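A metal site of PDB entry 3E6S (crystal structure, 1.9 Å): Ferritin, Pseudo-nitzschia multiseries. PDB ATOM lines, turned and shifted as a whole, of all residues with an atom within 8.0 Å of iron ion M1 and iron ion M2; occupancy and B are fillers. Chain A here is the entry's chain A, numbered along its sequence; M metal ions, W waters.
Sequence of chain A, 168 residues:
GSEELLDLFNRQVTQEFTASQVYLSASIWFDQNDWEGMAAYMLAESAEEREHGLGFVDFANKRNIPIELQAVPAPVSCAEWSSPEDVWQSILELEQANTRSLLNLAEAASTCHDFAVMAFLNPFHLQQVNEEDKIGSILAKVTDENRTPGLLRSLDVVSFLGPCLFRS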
ATOM      1  N   GLU A  16     -10.283 -19.518  17.348  1.00  0.00           N
ATOM      2  CA  GLU A  16      -9.078 -20.320  17.125  1.00  0.00           C
ATOM      3  C   GLU A  16      -8.979 -20.757  15.646  1.00  0.00           C
ATOM      4  O   GLU A  16      -7.895 -20.709  15.051  1.00  0.00           O
ATOM      5  CB  GLU A  16      -9.077 -21.566  18.015  1.00  0.00           C
ATOM      6  CG  GLU A  16      -9.075 -21.307  19.561  1.00  0.00           C
ATOM      7  CD  GLU A  16      -7.864 -20.472  20.000  1.00  0.00           C
ATOM      8  OE1 GLU A  16      -6.794 -20.568  19.337  1.00  0.00           O
ATOM      9  OE2 GLU A  16      -7.983 -19.707  20.996  1.00  0.00           O
ATOM     10  N   ALA A  19      -8.131 -17.716  13.520  1.00  0.00           N
ATOM     11  CA  ALA A  19      -6.702 -17.432  13.671  1.00  0.00           C
ATOM     12  C   ALA A  19      -5.876 -18.421  12.852  1.00  0.00           C
ATOM     13  O   ALA A  19      -4.916 -18.026  12.203  1.00  0.00           O
ATOM     14  CB  ALA A  19      -6.294 -17.523  15.161  1.00  0.00           C
ATOM     15  N   SER A  20      -6.223 -19.707  12.927  1.00  0.00           N
ATOM     16  CA  SER A  20      -5.574 -20.714  12.090  1.00  0.00           C
ATOM     17  C   SER A  20      -5.497 -20.289  10.602  1.00  0.00           C
ATOM     18  O   SER A  20      -4.453 -20.466   9.943  1.00  0.00           O
ATOM     19  CB  SER A  20      -6.314 -22.064  12.198  1.00  0.00           C
ATOM     20  OG  SER A  20      -5.533 -23.073  11.572  1.00  0.00           O
ATOM     21  N   TYR A  23      -3.201 -17.267  10.022  1.00  0.00           N
ATOM     22  CA  TYR A  23      -1.822 -17.765  10.004  1.00  0.00           C
ATOM     23  C   TYR A  23      -1.510 -18.453   8.665  1.00  0.00           C
ATOM     24  O   TYR A  23      -0.426 -18.282   8.112  1.00  0.00           O
ATOM     25  CB  TYR A  23      -1.589 -18.720  11.155  1.00  0.00           C
ATOM     26  CG  TYR A  23      -1.174 -18.021  12.431  1.00  0.00           C
ATOM     27  CD1 TYR A  23      -1.961 -18.052  13.563  1.00  0.00           C
ATOM     28  CD2 TYR A  23       0.066 -17.378  12.493  1.00  0.00           C
ATOM     29  CE1 TYR A  23      -1.529 -17.419  14.779  1.00  0.00           C
ATOM     30  CE2 TYR A  23       0.515 -16.770  13.655  1.00  0.00           C
ATOM     31  CZ  TYR A  23      -0.273 -16.800  14.788  1.00  0.00           C
ATOM     32  OH  TYR A  23       0.215 -16.157  15.901  1.00  0.00           O
ATOM     33  N   TYR A  41       7.123 -20.699  10.142  1.00  0.00           N
ATOM     34  CA  TYR A  41       6.672 -20.294  11.455  1.00  0.00           C
ATOM     35  C   TYR A  41       5.154 -20.083  11.438  1.00  0.00           C
ATOM     36  O   TYR A  41       4.440 -20.463  12.383  1.00  0.00           O
ATOM     37  CB  TYR A  41       7.305 -18.961  11.863  1.00  0.00           C
ATOM     38  CG  TYR A  41       7.029 -18.564  13.289  1.00  0.00           C
ATOM     39  CD1 TYR A  41       7.972 -18.800  14.262  1.00  0.00           C
ATOM     40  CD2 TYR A  41       5.864 -17.879  13.645  1.00  0.00           C
ATOM     41  CE1 TYR A  41       7.767 -18.424  15.556  1.00  0.00           C
ATOM     42  CE2 TYR A  41       5.640 -17.493  14.975  1.00  0.00           C
ATOM     43  CZ  TYR A  41       6.620 -17.791  15.911  1.00  0.00           C
ATOM     44  OH  TYR A  41       6.510 -17.458  17.244  1.00  0.00           O
ATOM     45  N   ALA A  44       3.351 -23.482  11.257  1.00  0.00           N
ATOM     46  CA  ALA A  44       3.356 -24.108  12.581  1.00  0.00           C
ATOM     47  C   ALA A  44       2.264 -23.510  13.481  1.00  0.00           C
ATOM     48  O   ALA A  44       1.516 -24.250  14.142  1.00  0.00           O
ATOM     49  CB  ALA A  44       4.753 -23.916  13.253  1.00  0.00           C
ATOM     50  N   GLU A  45       2.140 -22.192  13.510  1.00  0.00           N
ATOM     51  CA  GLU A  45       1.066 -21.554  14.323  1.00  0.00           C
ATOM     52  C   GLU A  45      -0.321 -21.863  13.802  1.00  0.00           C
ATOM     53  O   GLU A  45      -1.264 -21.948  14.589  1.00  0.00           O
ATOM     54  CB  GLU A  45       1.205 -20.033  14.307  1.00  0.00           C
ATOM     55  CG  GLU A  45       2.157 -19.502  15.331  1.00  0.00           C
ATOM     56  CD  GLU A  45       1.604 -19.709  16.708  1.00  0.00           C
ATOM     57  OE1 GLU A  45       0.501 -19.165  17.026  1.00  0.00           O
ATOM     58  OE2 GLU A  45       2.257 -20.477  17.445  1.00  0.00           O
ATOM     59  N   SER A  46      -0.479 -21.967  12.480  1.00  0.00           N
ATOM     60  CA  SER A  46      -1.782 -22.347  11.910  1.00  0.00           C
ATOM     61  C   SER A  46      -2.223 -23.723  12.443  1.00  0.00           C
ATOM     62  O   SER A  46      -3.386 -23.918  12.832  1.00  0.00           O
ATOM     63  CB  SER A  46      -1.716 -22.352  10.369  1.00  0.00           C
ATOM     64  OG  SER A  46      -2.951 -22.779   9.804  1.00  0.00           O
ATOM     65  N   GLU A  48      -1.079 -25.191  15.250  1.00  0.00           N
ATOM     66  CA  GLU A  48      -1.281 -25.061  16.663  1.00  0.00           C
ATOM     67  C   GLU A  48      -2.602 -24.363  17.035  1.00  0.00           C
ATOM     68  O   GLU A  48      -3.258 -24.809  17.979  1.00  0.00           O
ATOM     69  CB  GLU A  48      -0.127 -24.313  17.285  1.00  0.00           C
ATOM     70  CG  GLU A  48      -0.348 -23.965  18.715  1.00  0.00           C
ATOM     71  CD  GLU A  48       0.956 -23.967  19.452  1.00  0.00           C
ATOM     72  OE1 GLU A  48       1.980 -23.627  18.810  1.00  0.00           O
ATOM     73  OE2 GLU A  48       0.963 -24.362  20.652  1.00  0.00           O
ATOM     74  N   GLU A  49      -2.997 -23.292  16.334  1.00  0.00           N
ATOM     75  CA  GLU A  49      -4.269 -22.663  16.619  1.00  0.00           C
ATOM     76  C   GLU A  49      -5.418 -23.642  16.379  1.00  0.00           C
ATOM     77  O   GLU A  49      -6.400 -23.677  17.154  1.00  0.00           O
ATOM     78  CB  GLU A  49      -4.547 -21.420  15.745  1.00  0.00           C
ATOM     79  CG  GLU A  49      -3.637 -20.235  15.944  1.00  0.00           C
ATOM     80  CD  GLU A  49      -3.631 -19.691  17.346  1.00  0.00           C
ATOM     81  OE1 GLU A  49      -4.673 -19.654  18.002  1.00  0.00           O
ATOM     82  OE2 GLU A  49      -2.568 -19.274  17.795  1.00  0.00           O
ATOM     83  N   ARG A  50      -5.318 -24.391  15.289  1.00  0.00           N
ATOM     84  CA  ARG A  50      -6.304 -25.447  15.044  1.00  0.00           C
ATOM     85  C   ARG A  50      -6.338 -26.445  16.217  1.00  0.00           C
ATOM     86  O   ARG A  50      -7.419 -26.839  16.688  1.00  0.00           O
ATOM     87  CB  ARG A  50      -6.013 -26.177  13.728  1.00  0.00           C
ATOM     88  CG  ARG A  50      -6.951 -27.374  13.551  1.00  0.00           C
ATOM     89  CD  ARG A  50      -7.047 -27.812  12.067  1.00  0.00           C
ATOM     90  NE  ARG A  50      -8.021 -28.918  11.906  1.00  0.00           N
ATOM     91  CZ  ARG A  50      -7.738 -30.174  12.261  1.00  0.00           C
ATOM     92  NH1 ARG A  50      -6.548 -30.488  12.783  1.00  0.00           N
ATOM     93  NH2 ARG A  50      -8.633 -31.116  12.128  1.00  0.00           N
ATOM     94  N   HIS A  52      -5.547 -25.961  19.343  1.00  0.00           N
ATOM     95  CA  HIS A  52      -6.275 -25.293  20.439  1.00  0.00           C
ATOM     96  C   HIS A  52      -7.791 -25.368  20.235  1.00  0.00           C
ATOM     97  O   HIS A  52      -8.521 -25.646  21.194  1.00  0.00           O
ATOM     98  CB  HIS A  52      -5.889 -23.811  20.557  1.00  0.00           C
ATOM     99  CG  HIS A  52      -4.482 -23.602  20.988  1.00  0.00           C
ATOM    100  ND1 HIS A  52      -3.669 -24.621  21.429  1.00  0.00           N
ATOM    101  CD2 HIS A  52      -3.712 -22.482  20.987  1.00  0.00           C
ATOM    102  CE1 HIS A  52      -2.472 -24.139  21.713  1.00  0.00           C
ATOM    103  NE2 HIS A  52      -2.471 -22.847  21.448  1.00  0.00           N
ATOM    104  N   ILE A  91      -0.334 -10.217  12.695  1.00  0.00           N
ATOM    105  CA  ILE A  91      -0.234 -11.441  13.549  1.00  0.00           C
ATOM    106  C   ILE A  91      -0.233 -11.068  15.053  1.00  0.00           C
ATOM    107  O   ILE A  91      -0.898 -11.708  15.894  1.00  0.00           O
ATOM    108  CB  ILE A  91       1.040 -12.289  13.191  1.00  0.00           C
ATOM    109  CG1 ILE A  91       0.904 -12.902  11.795  1.00  0.00           C
ATOM    110  CG2 ILE A  91       1.268 -13.418  14.231  1.00  0.00           C
ATOM    111  CD1 ILE A  91      -0.425 -13.582  11.541  1.00  0.00           C
ATOM    112  N   LEU A  94      -3.702 -10.155  15.983  1.00  0.00           N
ATOM    113  CA  LEU A  94      -4.499 -11.396  16.023  1.00  0.00           C
ATOM    114  C   LEU A  94      -4.344 -12.052  17.389  1.00  0.00           C
ATOM    115  O   LEU A  94      -5.343 -12.442  18.052  1.00  0.00           O
ATOM    116  CB  LEU A  94      -3.980 -12.359  14.905  1.00  0.00           C
ATOM    117  CG  LEU A  94      -4.717 -13.702  14.808  1.00  0.00           C
ATOM    118  CD1 LEU A  94      -6.164 -13.419  14.336  1.00  0.00           C
ATOM    119  CD2 LEU A  94      -3.959 -14.684  13.881  1.00  0.00           C
ATOM    120  N   GLU A  95      -3.101 -12.186  17.833  1.00  0.00           N
ATOM    121  CA  GLU A  95      -2.852 -12.827  19.132  1.00  0.00           C
ATOM    122  C   GLU A  95      -3.366 -11.958  20.283  1.00  0.00           C
ATOM    123  O   GLU A  95      -3.847 -12.487  21.281  1.00  0.00           O
ATOM    124  CB  GLU A  95      -1.379 -13.147  19.332  1.00  0.00           C
ATOM    125  CG  GLU A  95      -0.895 -14.314  18.443  1.00  0.00           C
ATOM    126  CD  GLU A  95      -1.495 -15.655  18.824  1.00  0.00           C
ATOM    127  OE1 GLU A  95      -2.227 -15.741  19.844  1.00  0.00           O
ATOM    128  OE2 GLU A  95      -1.230 -16.628  18.092  1.00  0.00           O
ATOM    129  N   ASN A  98      -6.914 -12.767  20.367  1.00  0.00           N
ATOM    130  CA  ASN A  98      -6.995 -14.118  20.963  1.00  0.00           C
ATOM    131  C   ASN A  98      -6.940 -14.042  22.527  1.00  0.00           C
ATOM    132  O   ASN A  98      -7.720 -14.677  23.221  1.00  0.00           O
ATOM    133  CB  ASN A  98      -5.841 -15.043  20.466  1.00  0.00           C
ATOM    134  CG  ASN A  98      -6.054 -15.659  19.039  1.00  0.00           C
ATOM    135  OD1 ASN A  98      -7.122 -15.580  18.424  1.00  0.00           O
ATOM    136  ND2 ASN A  98      -4.988 -16.276  18.528  1.00  0.00           N
ATOM    137  N   GLN A 127       0.031 -19.487  28.051  1.00  0.00           N
ATOM    138  CA  GLN A 127       0.509 -19.600  26.681  1.00  0.00           C
ATOM    139  C   GLN A 127       0.355 -18.283  25.894  1.00  0.00           C
ATOM    140  O   GLN A 127       1.266 -17.922  25.122  1.00  0.00           O
ATOM    141  CB  GLN A 127      -0.202 -20.764  25.989  1.00  0.00           C
ATOM    142  CG  GLN A 127       0.129 -20.979  24.549  1.00  0.00           C
ATOM    143  CD  GLN A 127      -0.512 -22.263  23.973  1.00  0.00           C
ATOM    144  OE1 GLN A 127      -1.465 -22.841  24.560  1.00  0.00           O
ATOM    145  NE2 GLN A 127       0.019 -22.715  22.837  1.00  0.00           N
ATOM    146  N   GLN A 128      -0.744 -17.560  26.096  1.00  0.00           N
ATOM    147  CA  GLN A 128      -0.918 -16.271  25.391  1.00  0.00           C
ATOM    148  C   GLN A 128       0.132 -15.262  25.821  1.00  0.00           C
ATOM    149  O   GLN A 128       0.657 -14.519  24.999  1.00  0.00           O
ATOM    150  CB  GLN A 128      -2.312 -15.657  25.579  1.00  0.00           C
ATOM    151  CG  GLN A 128      -3.390 -16.347  24.808  1.00  0.00           C
ATOM    152  CD  GLN A 128      -3.029 -16.457  23.324  1.00  0.00           C
ATOM    153  OE1 GLN A 128      -2.638 -17.520  22.877  1.00  0.00           O
ATOM    154  NE2 GLN A 128      -3.043 -15.334  22.604  1.00  0.00           N
ATOM    155  N   ASN A 130       3.247 -15.912  26.793  1.00  0.00           N
ATOM    156  CA  ASN A 130       4.473 -16.286  26.111  1.00  0.00           C
ATOM    157  C   ASN A 130       4.436 -15.940  24.635  1.00  0.00           C
ATOM    158  O   ASN A 130       5.423 -15.490  24.077  1.00  0.00           O
ATOM    159  CB  ASN A 130       4.733 -17.773  26.234  1.00  0.00           C
ATOM    160  CG  ASN A 130       5.080 -18.192  27.640  1.00  0.00           C
ATOM    161  OD1 ASN A 130       5.433 -17.358  28.495  1.00  0.00           O
ATOM    162  ND2 ASN A 130       4.969 -19.508  27.898  1.00  0.00           N
ATOM    163  N   GLU A 131       3.294 -16.177  23.994  1.00  0.00           N
ATOM    164  CA  GLU A 131       3.207 -15.975  22.552  1.00  0.00           C
ATOM    165  C   GLU A 131       3.215 -14.510  22.152  1.00  0.00           C
ATOM    166  O   GLU A 131       3.846 -14.136  21.155  1.00  0.00           O
ATOM    167  CB  GLU A 131       1.924 -16.558  22.024  1.00  0.00           C
ATOM    168  CG  GLU A 131       1.941 -17.986  21.761  1.00  0.00           C
ATOM    169  CD  GLU A 131       0.862 -18.275  20.751  1.00  0.00           C
ATOM    170  OE1 GLU A 131       1.110 -17.981  19.558  1.00  0.00           O
ATOM    171  OE2 GLU A 131      -0.231 -18.727  21.156  1.00  0.00           O
ATOM    172  N   GLU A 132       2.465 -13.674  22.875  1.00  0.00           N
ATOM    173  CA  GLU A 132       2.469 -12.252  22.586  1.00  0.00           C
ATOM    174  C   GLU A 132       3.876 -11.672  22.758  1.00  0.00           C
ATOM    175  O   GLU A 132       4.289 -10.798  21.992  1.00  0.00           O
ATOM    176  CB  GLU A 132       1.491 -11.520  23.497  1.00  0.00           C
ATOM    177  CG  GLU A 132       0.014 -11.577  23.077  1.00  0.00           C
ATOM    178  CD  GLU A 132      -0.836 -10.554  23.817  1.00  0.00           C
ATOM    179  OE1 GLU A 132      -0.313  -9.454  24.131  1.00  0.00           O
ATOM    180  OE2 GLU A 132      -2.028 -10.806  24.051  1.00  0.00           O
ATOM    181  N   LYS A 134       6.743 -13.327  22.350  1.00  0.00           N
ATOM    182  CA  LYS A 134       7.574 -13.826  21.219  1.00  0.00           C
ATOM    183  C   LYS A 134       7.262 -13.066  19.923  1.00  0.00           C
ATOM    184  O   LYS A 134       8.176 -12.604  19.212  1.00  0.00           O
ATOM    185  CB  LYS A 134       7.386 -15.322  21.006  1.00  0.00           C
ATOM    186  CG  LYS A 134       8.064 -16.269  22.087  1.00  0.00           C
ATOM    187  CD  LYS A 134       9.441 -15.738  22.571  1.00  0.00           C
ATOM    188  CE  LYS A 134      10.546 -16.802  22.663  1.00  0.00           C
ATOM    189  NZ  LYS A 134      11.872 -16.155  22.970  1.00  0.00           N
ATOM    190  N   ILE A 135       5.963 -12.909  19.612  1.00  0.00           N
ATOM    191  CA  ILE A 135       5.567 -12.186  18.381  1.00  0.00           C
ATOM    192  C   ILE A 135       5.972 -10.714  18.462  1.00  0.00           C
ATOM    193  O   ILE A 135       6.464 -10.137  17.481  1.00  0.00           O
ATOM    194  CB  ILE A 135       4.067 -12.341  18.100  1.00  0.00           C
ATOM    195  CG1 ILE A 135       3.768 -13.801  17.773  1.00  0.00           C
ATOM    196  CG2 ILE A 135       3.630 -11.455  16.956  1.00  0.00           C
ATOM    197  CD1 ILE A 135       2.351 -14.147  17.999  1.00  0.00           C
HETATM  198 FE    FE M   1      -0.958 -18.697  18.702  1.00  0.00          FE
HETATM  199 FE    FE M   2       1.940 -20.823  19.364  1.00  0.00          FE
HETATM  200 FE    FE M   3       3.201 -23.233  21.151  1.00  0.00          FE
HETATM  201  O   HOH W   1      -2.429 -18.575  20.263  1.00  0.00           O
HETATM  202  O   HOH W   2      -0.658 -20.698  19.313  1.00  0.00           O
HETATM  203  O   HOH W   3       3.948 -21.981  19.271  1.00  0.00           O
HETATM  204  O   HOH W   4       1.715 -21.638  21.600  1.00  0.00           O
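The side-chain carboxylate (OE1) of Glu 49 lies within hydrogen-bond range of the side-chain amide nitrogen (ND2) of Asn 98 (3.4 Å).
OH of Tyr 23 sits close to OE1 of Glu 45, at 3.2 Å.
The side-chain carboxylate of Glu 95 sits close to the side-chain hydroxyl of Tyr 23, 2.7 Å away.
OE1 of Glu 95 sits at hydrogen-bond distance from NE2 of Gln 128, at 2.9 Å.
The side-chain carboxylate (OE1) of Glu 95 sits at hydrogen-bond distance from the side-chain amide nitrogen (ND2) of Asn 98 (3.1 Å).
The side-chain carboxylate (OE2) of Glu 131 lies close to the side-chain amide oxygen (OE1) of Gln 128, at 3.2 Å.
The side-chain carboxylate (OE2) of Glu 48 lies close to the side-chain amide nitrogen (NE2) of Gln 127, 2.9 Å away.
ND1 of His 52 sits close to O of Glu 48.
Merely in contact with iron ion M1: Tyr 23 (3.96 Å).
The nearest printed residue that does not touch iron ion M1 is Gln 128 (4.7 Å).
Glu 48 touches iron ion M2 (OE1 to FE, 2.9 Å).
The nearest printed residue that does not touch iron ion M2 is Gln 127 (4.4 Å).
Iron ion M1 is bound by the side-chain carboxylate (OE2) of Glu 49 (1.9 Å), water W2 (2.1 Å), water W1 (2.1 Å), the side-chain carboxylate (OE2) of Glu 95 (2.2 Å), the side-chain carboxylate (OE1) of Glu 45 (2.3 Å), the side-chain carboxylate (OE1) of Glu 131 (2.3 Å) and the side-chain carboxylate (OE2) of Glu 131 (2.6 Å).
OE2 of Glu 45 binds iron ion M2 (2.0 Å).
Water W3 is bound to iron ion M2, at 2.3 Å.
Iron ion M2 is bound by water W4 (2.4 Å).
Water W2 binds iron ion M2 (2.6 Å).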
